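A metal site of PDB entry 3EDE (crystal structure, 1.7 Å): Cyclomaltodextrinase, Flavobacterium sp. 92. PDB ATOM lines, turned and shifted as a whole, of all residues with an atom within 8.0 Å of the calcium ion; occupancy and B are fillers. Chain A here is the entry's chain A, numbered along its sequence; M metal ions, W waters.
The calcium ion is bound by the side-chain hydroxyl (OG) of Ser 222 (2.4 Å), the backbone carbonyl oxygen (O) of Tyr 315 (2.4 Å), water W1 (2.4 Å), water W2 (2.4 Å), the backbone carbonyl oxygen (O) of Thr 270 (2.4 Å), the side-chain carboxylate (OD2) of Asp 280 (2.5 Å) and the side-chain carboxylate (OD1) of Asp 280 (2.5 Å). The calcium ion has seven donor atoms within binding distance.
OG of Ser 316 lies within hydrogen-bond range of N of Ser 222 (3.4 Å). O of Ser 222 sits at hydrogen-bond distance from N of Leu 281. O of Asp 280 is in hydrogen-bond range of N of Asn 241 (2.8 Å).
Four residues have an atom within 4 Å of the calcium ion: Ser 222, Thr 270, Asp 280 and Tyr 315. The nearest printed residue that does not touch the calcium ion is Lys 271 (4.1 Å).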
ATOM      1  N   LEU A 221       4.284 -13.682 -25.817  1.00  0.00           N
ATOM      2  CA  LEU A 221       3.005 -13.076 -25.374  1.00  0.00           C
ATOM      3  C   LEU A 221       3.162 -11.601 -25.000  1.00  0.00           C
ATOM      4  O   LEU A 221       2.209 -10.806 -25.191  1.00  0.00           O
ATOM      5  CB  LEU A 221       2.461 -13.841 -24.155  1.00  0.00           C
ATOM      6  CG  LEU A 221       2.219 -15.355 -24.340  1.00  0.00           C
ATOM      7  CD1 LEU A 221       1.791 -15.988 -22.989  1.00  0.00           C
ATOM      8  CD2 LEU A 221       1.184 -15.553 -25.421  1.00  0.00           C
ATOM      9  N   SER A 222       4.341 -11.216 -24.478  1.00  0.00           N
ATOM     10  CA  SER A 222       4.553  -9.884 -23.931  1.00  0.00           C
ATOM     11  C   SER A 222       4.699  -8.757 -24.972  1.00  0.00           C
ATOM     12  O   SER A 222       4.308  -7.592 -24.699  1.00  0.00           O
ATOM     13  CB  SER A 222       5.788  -9.908 -23.011  1.00  0.00           C
ATOM     14  OG  SER A 222       6.120  -8.637 -22.466  1.00  0.00           O
ATOM     15  N   HIS A 223       5.309  -9.098 -26.102  1.00  0.00           N
ATOM     16  CA  HIS A 223       5.694  -8.075 -27.097  1.00  0.00           C
ATOM     17  C   HIS A 223       5.556  -8.507 -28.554  1.00  0.00           C
ATOM     18  O   HIS A 223       5.334  -9.687 -28.877  1.00  0.00           O
ATOM     19  CB  HIS A 223       7.144  -7.596 -26.836  1.00  0.00           C
ATOM     20  CG  HIS A 223       8.173  -8.680 -26.963  1.00  0.00           C
ATOM     21  ND1 HIS A 223       8.641  -9.391 -25.881  1.00  0.00           N
ATOM     22  CD2 HIS A 223       8.781  -9.200 -28.052  1.00  0.00           C
ATOM     23  CE1 HIS A 223       9.528 -10.277 -26.289  1.00  0.00           C
ATOM     24  NE2 HIS A 223       9.620 -10.198 -27.604  1.00  0.00           N
ATOM     25  N   ASN A 241       1.528  -0.778 -24.270  1.00  0.00           N
ATOM     26  CA  ASN A 241       1.888  -0.105 -23.022  1.00  0.00           C
ATOM     27  C   ASN A 241       2.597   1.228 -23.263  1.00  0.00           C
ATOM     28  O   ASN A 241       3.353   1.381 -24.232  1.00  0.00           O
ATOM     29  CB  ASN A 241       2.733  -1.018 -22.138  1.00  0.00           C
ATOM     30  CG  ASN A 241       1.911  -2.084 -21.448  1.00  0.00           C
ATOM     31  OD1 ASN A 241       2.261  -3.279 -21.485  1.00  0.00           O
ATOM     32  ND2 ASN A 241       0.804  -1.680 -20.842  1.00  0.00           N
ATOM     33  N   THR A 249      12.003  -1.504 -20.050  1.00  0.00           N
ATOM     34  CA  THR A 249      12.078  -2.249 -18.796  1.00  0.00           C
ATOM     35  C   THR A 249      13.524  -2.269 -18.273  1.00  0.00           C
ATOM     36  O   THR A 249      14.508  -2.264 -19.069  1.00  0.00           O
ATOM     37  CB  THR A 249      11.583  -3.720 -18.956  1.00  0.00           C
ATOM     38  OG1 THR A 249      11.511  -4.310 -17.653  1.00  0.00           O
ATOM     39  CG2 THR A 249      12.570  -4.565 -19.834  1.00  0.00           C
ATOM     40  N   GLU A 267       5.253  -2.875 -12.365  1.00  0.00           N
ATOM     41  CA  GLU A 267       4.761  -2.306 -13.607  1.00  0.00           C
ATOM     42  C   GLU A 267       5.855  -2.195 -14.668  1.00  0.00           C
ATOM     43  O   GLU A 267       5.627  -2.487 -15.836  1.00  0.00           O
ATOM     44  CB  GLU A 267       4.161  -0.933 -13.328  1.00  0.00           C
ATOM     45  CG  GLU A 267       2.936  -1.068 -12.450  1.00  0.00           C
ATOM     46  CD  GLU A 267       1.805  -1.759 -13.174  1.00  0.00           C
ATOM     47  OE1 GLU A 267       1.361  -2.838 -12.732  1.00  0.00           O
ATOM     48  OE2 GLU A 267       1.396  -1.234 -14.237  1.00  0.00           O
ATOM     49  N   ASN A 268       7.063  -1.793 -14.262  1.00  0.00           N
ATOM     50  CA  ASN A 268       8.140  -1.672 -15.211  1.00  0.00           C
ATOM     51  C   ASN A 268       8.524  -3.026 -15.793  1.00  0.00           C
ATOM     52  O   ASN A 268       8.930  -3.108 -16.927  1.00  0.00           O
ATOM     53  CB  ASN A 268       9.355  -0.973 -14.587  1.00  0.00           C
ATOM     54  CG  ASN A 268      10.509  -0.863 -15.544  1.00  0.00           C
ATOM     55  OD1 ASN A 268      11.425  -1.659 -15.482  1.00  0.00           O
ATOM     56  ND2 ASN A 268      10.478   0.122 -16.470  1.00  0.00           N
ATOM     57  N   PHE A 269       8.384  -4.077 -14.999  1.00  0.00           N
ATOM     58  CA  PHE A 269       8.743  -5.400 -15.497  1.00  0.00           C
ATOM     59  C   PHE A 269       7.736  -5.906 -16.509  1.00  0.00           C
ATOM     60  O   PHE A 269       8.135  -6.492 -17.516  1.00  0.00           O
ATOM     61  CB  PHE A 269       8.878  -6.426 -14.381  1.00  0.00           C
ATOM     62  CG  PHE A 269       9.538  -7.716 -14.842  1.00  0.00           C
ATOM     63  CD1 PHE A 269      10.878  -7.700 -15.248  1.00  0.00           C
ATOM     64  CD2 PHE A 269       8.835  -8.938 -14.833  1.00  0.00           C
ATOM     65  CE1 PHE A 269      11.516  -8.880 -15.688  1.00  0.00           C
ATOM     66  CE2 PHE A 269       9.483 -10.120 -15.256  1.00  0.00           C
ATOM     67  CZ  PHE A 269      10.816 -10.073 -15.700  1.00  0.00           C
ATOM     68  N   THR A 270       6.451  -5.691 -16.247  1.00  0.00           N
ATOM     69  CA  THR A 270       5.400  -6.275 -17.073  1.00  0.00           C
ATOM     70  C   THR A 270       4.915  -5.369 -18.218  1.00  0.00           C
ATOM     71  O   THR A 270       4.294  -5.861 -19.139  1.00  0.00           O
ATOM     72  CB  THR A 270       4.165  -6.748 -16.232  1.00  0.00           C
ATOM     73  OG1 THR A 270       3.479  -5.609 -15.668  1.00  0.00           O
ATOM     74  CG2 THR A 270       4.544  -7.734 -15.117  1.00  0.00           C
ATOM     75  N   LYS A 271       5.176  -4.049 -18.119  1.00  0.00           N
ATOM     76  CA  LYS A 271       4.775  -3.074 -19.133  1.00  0.00           C
ATOM     77  C   LYS A 271       5.960  -2.447 -19.865  1.00  0.00           C
ATOM     78  O   LYS A 271       5.839  -1.995 -20.996  1.00  0.00           O
ATOM     79  CB  LYS A 271       3.928  -1.938 -18.518  1.00  0.00           C
ATOM     80  CG  LYS A 271       2.592  -2.398 -17.906  1.00  0.00           C
ATOM     81  CD  LYS A 271       1.682  -1.189 -17.614  1.00  0.00           C
ATOM     82  CE  LYS A 271       0.213  -1.618 -17.452  1.00  0.00           C
ATOM     83  NZ  LYS A 271       0.052  -2.587 -16.331  1.00  0.00           N
ATOM     84  N   GLY A 272       7.133  -2.445 -19.204  1.00  0.00           N
ATOM     85  CA  GLY A 272       8.359  -1.968 -19.870  1.00  0.00           C
ATOM     86  C   GLY A 272       8.716  -2.673 -21.172  1.00  0.00           C
ATOM     87  O   GLY A 272       8.591  -3.912 -21.302  1.00  0.00           O
ATOM     88  N   TRP A 273       9.202  -1.897 -22.154  1.00  0.00           N
ATOM     89  CA  TRP A 273       9.583  -2.478 -23.435  1.00  0.00           C
ATOM     90  C   TRP A 273      10.901  -3.194 -23.329  1.00  0.00           C
ATOM     91  O   TRP A 273      11.896  -2.691 -22.812  1.00  0.00           O
ATOM     92  CB  TRP A 273       9.658  -1.427 -24.536  1.00  0.00           C
ATOM     93  CG  TRP A 273       8.376  -0.796 -24.942  1.00  0.00           C
ATOM     94  CD1 TRP A 273       7.254  -0.540 -24.172  1.00  0.00           C
ATOM     95  CD2 TRP A 273       8.095  -0.288 -26.245  1.00  0.00           C
ATOM     96  NE1 TRP A 273       6.305   0.094 -24.937  1.00  0.00           N
ATOM     97  CE2 TRP A 273       6.803   0.261 -26.210  1.00  0.00           C
ATOM     98  CE3 TRP A 273       8.834  -0.233 -27.441  1.00  0.00           C
ATOM     99  CZ2 TRP A 273       6.216   0.865 -27.318  1.00  0.00           C
ATOM    100  CZ3 TRP A 273       8.256   0.357 -28.544  1.00  0.00           C
ATOM    101  CH2 TRP A 273       6.963   0.912 -28.473  1.00  0.00           C
ATOM    102  N   PHE A 274      10.896  -4.413 -23.851  1.00  0.00           N
ATOM    103  CA  PHE A 274      12.078  -5.223 -23.727  1.00  0.00           C
ATOM    104  C   PHE A 274      13.245  -4.492 -24.382  1.00  0.00           C
ATOM    105  O   PHE A 274      14.313  -4.401 -23.783  1.00  0.00           O
ATOM    106  CB  PHE A 274      11.860  -6.614 -24.321  1.00  0.00           C
ATOM    107  CG  PHE A 274      12.830  -7.603 -23.806  1.00  0.00           C
ATOM    108  CD1 PHE A 274      14.115  -7.701 -24.341  1.00  0.00           C
ATOM    109  CD2 PHE A 274      12.486  -8.426 -22.734  1.00  0.00           C
ATOM    110  CE1 PHE A 274      15.032  -8.595 -23.845  1.00  0.00           C
ATOM    111  CE2 PHE A 274      13.393  -9.324 -22.210  1.00  0.00           C
ATOM    112  CZ  PHE A 274      14.671  -9.435 -22.788  1.00  0.00           C
ATOM    113  N   MET A 278      10.739  -3.560 -29.952  1.00  0.00           N
ATOM    114  CA  MET A 278       9.743  -4.558 -29.469  1.00  0.00           C
ATOM    115  C   MET A 278       8.609  -3.950 -28.626  1.00  0.00           C
ATOM    116  O   MET A 278       8.639  -4.068 -27.391  1.00  0.00           O
ATOM    117  CB  MET A 278      10.414  -5.696 -28.695  1.00  0.00           C
ATOM    118  CG  MET A 278      11.202  -6.634 -29.578  1.00  0.00           C
ATOM    119  SD  MET A 278      12.036  -7.873 -28.547  1.00  0.00           S
ATOM    120  CE  MET A 278      12.900  -8.662 -29.901  1.00  0.00           C
ATOM    121  N   PRO A 279       7.617  -3.318 -29.289  1.00  0.00           N
ATOM    122  CA  PRO A 279       6.476  -2.771 -28.515  1.00  0.00           C
ATOM    123  C   PRO A 279       5.825  -3.778 -27.581  1.00  0.00           C
ATOM    124  O   PRO A 279       5.607  -4.934 -27.960  1.00  0.00           O
ATOM    125  CB  PRO A 279       5.482  -2.333 -29.604  1.00  0.00           C
ATOM    126  CG  PRO A 279       6.345  -2.036 -30.810  1.00  0.00           C
ATOM    127  CD  PRO A 279       7.480  -3.063 -30.738  1.00  0.00           C
ATOM    128  N   ASP A 280       5.456  -3.303 -26.407  1.00  0.00           N
ATOM    129  CA  ASP A 280       4.966  -4.152 -25.328  1.00  0.00           C
ATOM    130  C   ASP A 280       3.455  -4.130 -25.271  1.00  0.00           C
ATOM    131  O   ASP A 280       2.846  -3.059 -25.165  1.00  0.00           O
ATOM    132  CB  ASP A 280       5.523  -3.694 -24.013  1.00  0.00           C
ATOM    133  CG  ASP A 280       5.438  -4.779 -22.967  1.00  0.00           C
ATOM    134  OD1 ASP A 280       4.459  -4.797 -22.174  1.00  0.00           O
ATOM    135  OD2 ASP A 280       6.326  -5.636 -22.964  1.00  0.00           O
ATOM    136  N   LEU A 281       2.845  -5.325 -25.343  1.00  0.00           N
ATOM    137  CA  LEU A 281       1.379  -5.410 -25.377  1.00  0.00           C
ATOM    138  C   LEU A 281       0.739  -5.190 -24.004  1.00  0.00           C
ATOM    139  O   LEU A 281       1.198  -5.722 -23.002  1.00  0.00           O
ATOM    140  CB  LEU A 281       0.966  -6.807 -25.892  1.00  0.00           C
ATOM    141  CG  LEU A 281       1.410  -7.170 -27.311  1.00  0.00           C
ATOM    142  CD1 LEU A 281       0.897  -8.545 -27.713  1.00  0.00           C
ATOM    143  CD2 LEU A 281       0.929  -6.119 -28.331  1.00  0.00           C
ATOM    144  N   ASN A 282      -0.325  -4.385 -23.963  1.00  0.00           N
ATOM    145  CA  ASN A 282      -1.027  -4.144 -22.714  1.00  0.00           C
ATOM    146  C   ASN A 282      -2.056  -5.233 -22.450  1.00  0.00           C
ATOM    147  O   ASN A 282      -3.226  -5.146 -22.921  1.00  0.00           O
ATOM    148  CB  ASN A 282      -1.736  -2.782 -22.788  1.00  0.00           C
ATOM    149  CG  ASN A 282      -2.542  -2.501 -21.559  1.00  0.00           C
ATOM    150  OD1 ASN A 282      -2.410  -3.189 -20.534  1.00  0.00           O
ATOM    151  ND2 ASN A 282      -3.407  -1.478 -21.638  1.00  0.00           N
ATOM    152  N   GLN A 283      -1.636  -6.263 -21.725  1.00  0.00           N
ATOM    153  CA  GLN A 283      -2.486  -7.410 -21.516  1.00  0.00           C
ATOM    154  C   GLN A 283      -3.551  -7.171 -20.437  1.00  0.00           C
ATOM    155  O   GLN A 283      -4.411  -8.061 -20.200  1.00  0.00           O
ATOM    156  CB  GLN A 283      -1.629  -8.638 -21.190  1.00  0.00           C
ATOM    157  CG  GLN A 283      -0.714  -9.067 -22.367  1.00  0.00           C
ATOM    158  CD  GLN A 283       0.573  -9.680 -21.882  1.00  0.00           C
ATOM    159  OE1 GLN A 283       1.067  -9.326 -20.827  1.00  0.00           O
ATOM    160  NE2 GLN A 283       1.123 -10.625 -22.651  1.00  0.00           N
ATOM    161  N   THR A 312       9.994 -15.288 -22.507  1.00  0.00           N
ATOM    162  CA  THR A 312       9.926 -14.063 -21.661  1.00  0.00           C
ATOM    163  C   THR A 312       8.735 -14.123 -20.680  1.00  0.00           C
ATOM    164  O   THR A 312       7.858 -13.248 -20.677  1.00  0.00           O
ATOM    165  CB  THR A 312       9.874 -12.712 -22.519  1.00  0.00           C
ATOM    166  OG1 THR A 312       9.001 -12.831 -23.645  1.00  0.00           O
ATOM    167  CG2 THR A 312      11.261 -12.345 -23.007  1.00  0.00           C
ATOM    168  N   TYR A 313       8.701 -15.198 -19.899  1.00  0.00           N
ATOM    169  CA  TYR A 313       7.432 -15.566 -19.292  1.00  0.00           C
ATOM    170  C   TYR A 313       6.836 -14.450 -18.357  1.00  0.00           C
ATOM    171  O   TYR A 313       5.663 -14.060 -18.503  1.00  0.00           O
ATOM    172  CB  TYR A 313       7.569 -16.895 -18.501  1.00  0.00           C
ATOM    173  CG  TYR A 313       6.209 -17.403 -18.085  1.00  0.00           C
ATOM    174  CD1 TYR A 313       5.367 -18.003 -19.035  1.00  0.00           C
ATOM    175  CD2 TYR A 313       5.737 -17.218 -16.782  1.00  0.00           C
ATOM    176  CE1 TYR A 313       4.085 -18.411 -18.698  1.00  0.00           C
ATOM    177  CE2 TYR A 313       4.450 -17.652 -16.410  1.00  0.00           C
ATOM    178  CZ  TYR A 313       3.639 -18.235 -17.386  1.00  0.00           C
ATOM    179  OH  TYR A 313       2.341 -18.633 -17.107  1.00  0.00           O
ATOM    180  N   GLY A 314       7.649 -14.000 -17.395  1.00  0.00           N
ATOM    181  CA  GLY A 314       7.109 -13.069 -16.360  1.00  0.00           C
ATOM    182  C   GLY A 314       6.946 -11.651 -16.879  1.00  0.00           C
ATOM    183  O   GLY A 314       6.500 -10.783 -16.128  1.00  0.00           O
ATOM    184  N   TYR A 315       7.382 -11.401 -18.134  1.00  0.00           N
ATOM    185  CA  TYR A 315       7.235 -10.050 -18.701  1.00  0.00           C
ATOM    186  C   TYR A 315       5.795  -9.773 -19.148  1.00  0.00           C
ATOM    187  O   TYR A 315       5.443  -8.666 -19.561  1.00  0.00           O
ATOM    188  CB  TYR A 315       8.159  -9.852 -19.892  1.00  0.00           C
ATOM    189  CG  TYR A 315       9.617  -9.813 -19.550  1.00  0.00           C
ATOM    190  CD1 TYR A 315      10.292  -8.593 -19.409  1.00  0.00           C
ATOM    191  CD2 TYR A 315      10.347 -10.999 -19.392  1.00  0.00           C
ATOM    192  CE1 TYR A 315      11.608  -8.520 -19.102  1.00  0.00           C
ATOM    193  CE2 TYR A 315      11.722 -10.950 -19.073  1.00  0.00           C
ATOM    194  CZ  TYR A 315      12.351  -9.712 -18.940  1.00  0.00           C
ATOM    195  OH  TYR A 315      13.691  -9.651 -18.647  1.00  0.00           O
ATOM    196  N   SER A 316       4.956 -10.791 -19.092  1.00  0.00           N
ATOM    197  CA  SER A 316       3.525 -10.564 -19.308  1.00  0.00           C
ATOM    198  C   SER A 316       2.836 -10.213 -17.999  1.00  0.00           C
ATOM    199  O   SER A 316       3.263 -10.596 -16.875  1.00  0.00           O
ATOM    200  CB  SER A 316       2.875 -11.814 -19.944  1.00  0.00           C
ATOM    201  OG  SER A 316       3.292 -11.940 -21.304  1.00  0.00           O
ATOM    202  N   ASP A 317       1.730  -9.465 -18.112  1.00  0.00           N
ATOM    203  CA  ASP A 317       0.908  -9.173 -16.942  1.00  0.00           C
ATOM    204  C   ASP A 317       0.550 -10.454 -16.178  1.00  0.00           C
ATOM    205  O   ASP A 317       0.077 -11.445 -16.770  1.00  0.00           O
ATOM    206  CB  ASP A 317      -0.401  -8.466 -17.349  1.00  0.00           C
ATOM    207  CG  ASP A 317      -1.213  -8.023 -16.158  1.00  0.00           C
ATOM    208  OD1 ASP A 317      -2.143  -8.752 -15.743  1.00  0.00           O
ATOM    209  OD2 ASP A 317      -0.898  -6.958 -15.577  1.00  0.00           O
HETATM  210 CA    CA M   1       5.265  -6.883 -21.128  1.00  0.00          CA
HETATM  211  O   HOH W   1       7.274  -5.981 -20.170  1.00  0.00           O
HETATM  212  O   HOH W   2       2.919  -7.342 -21.570  1.00  0.00           O
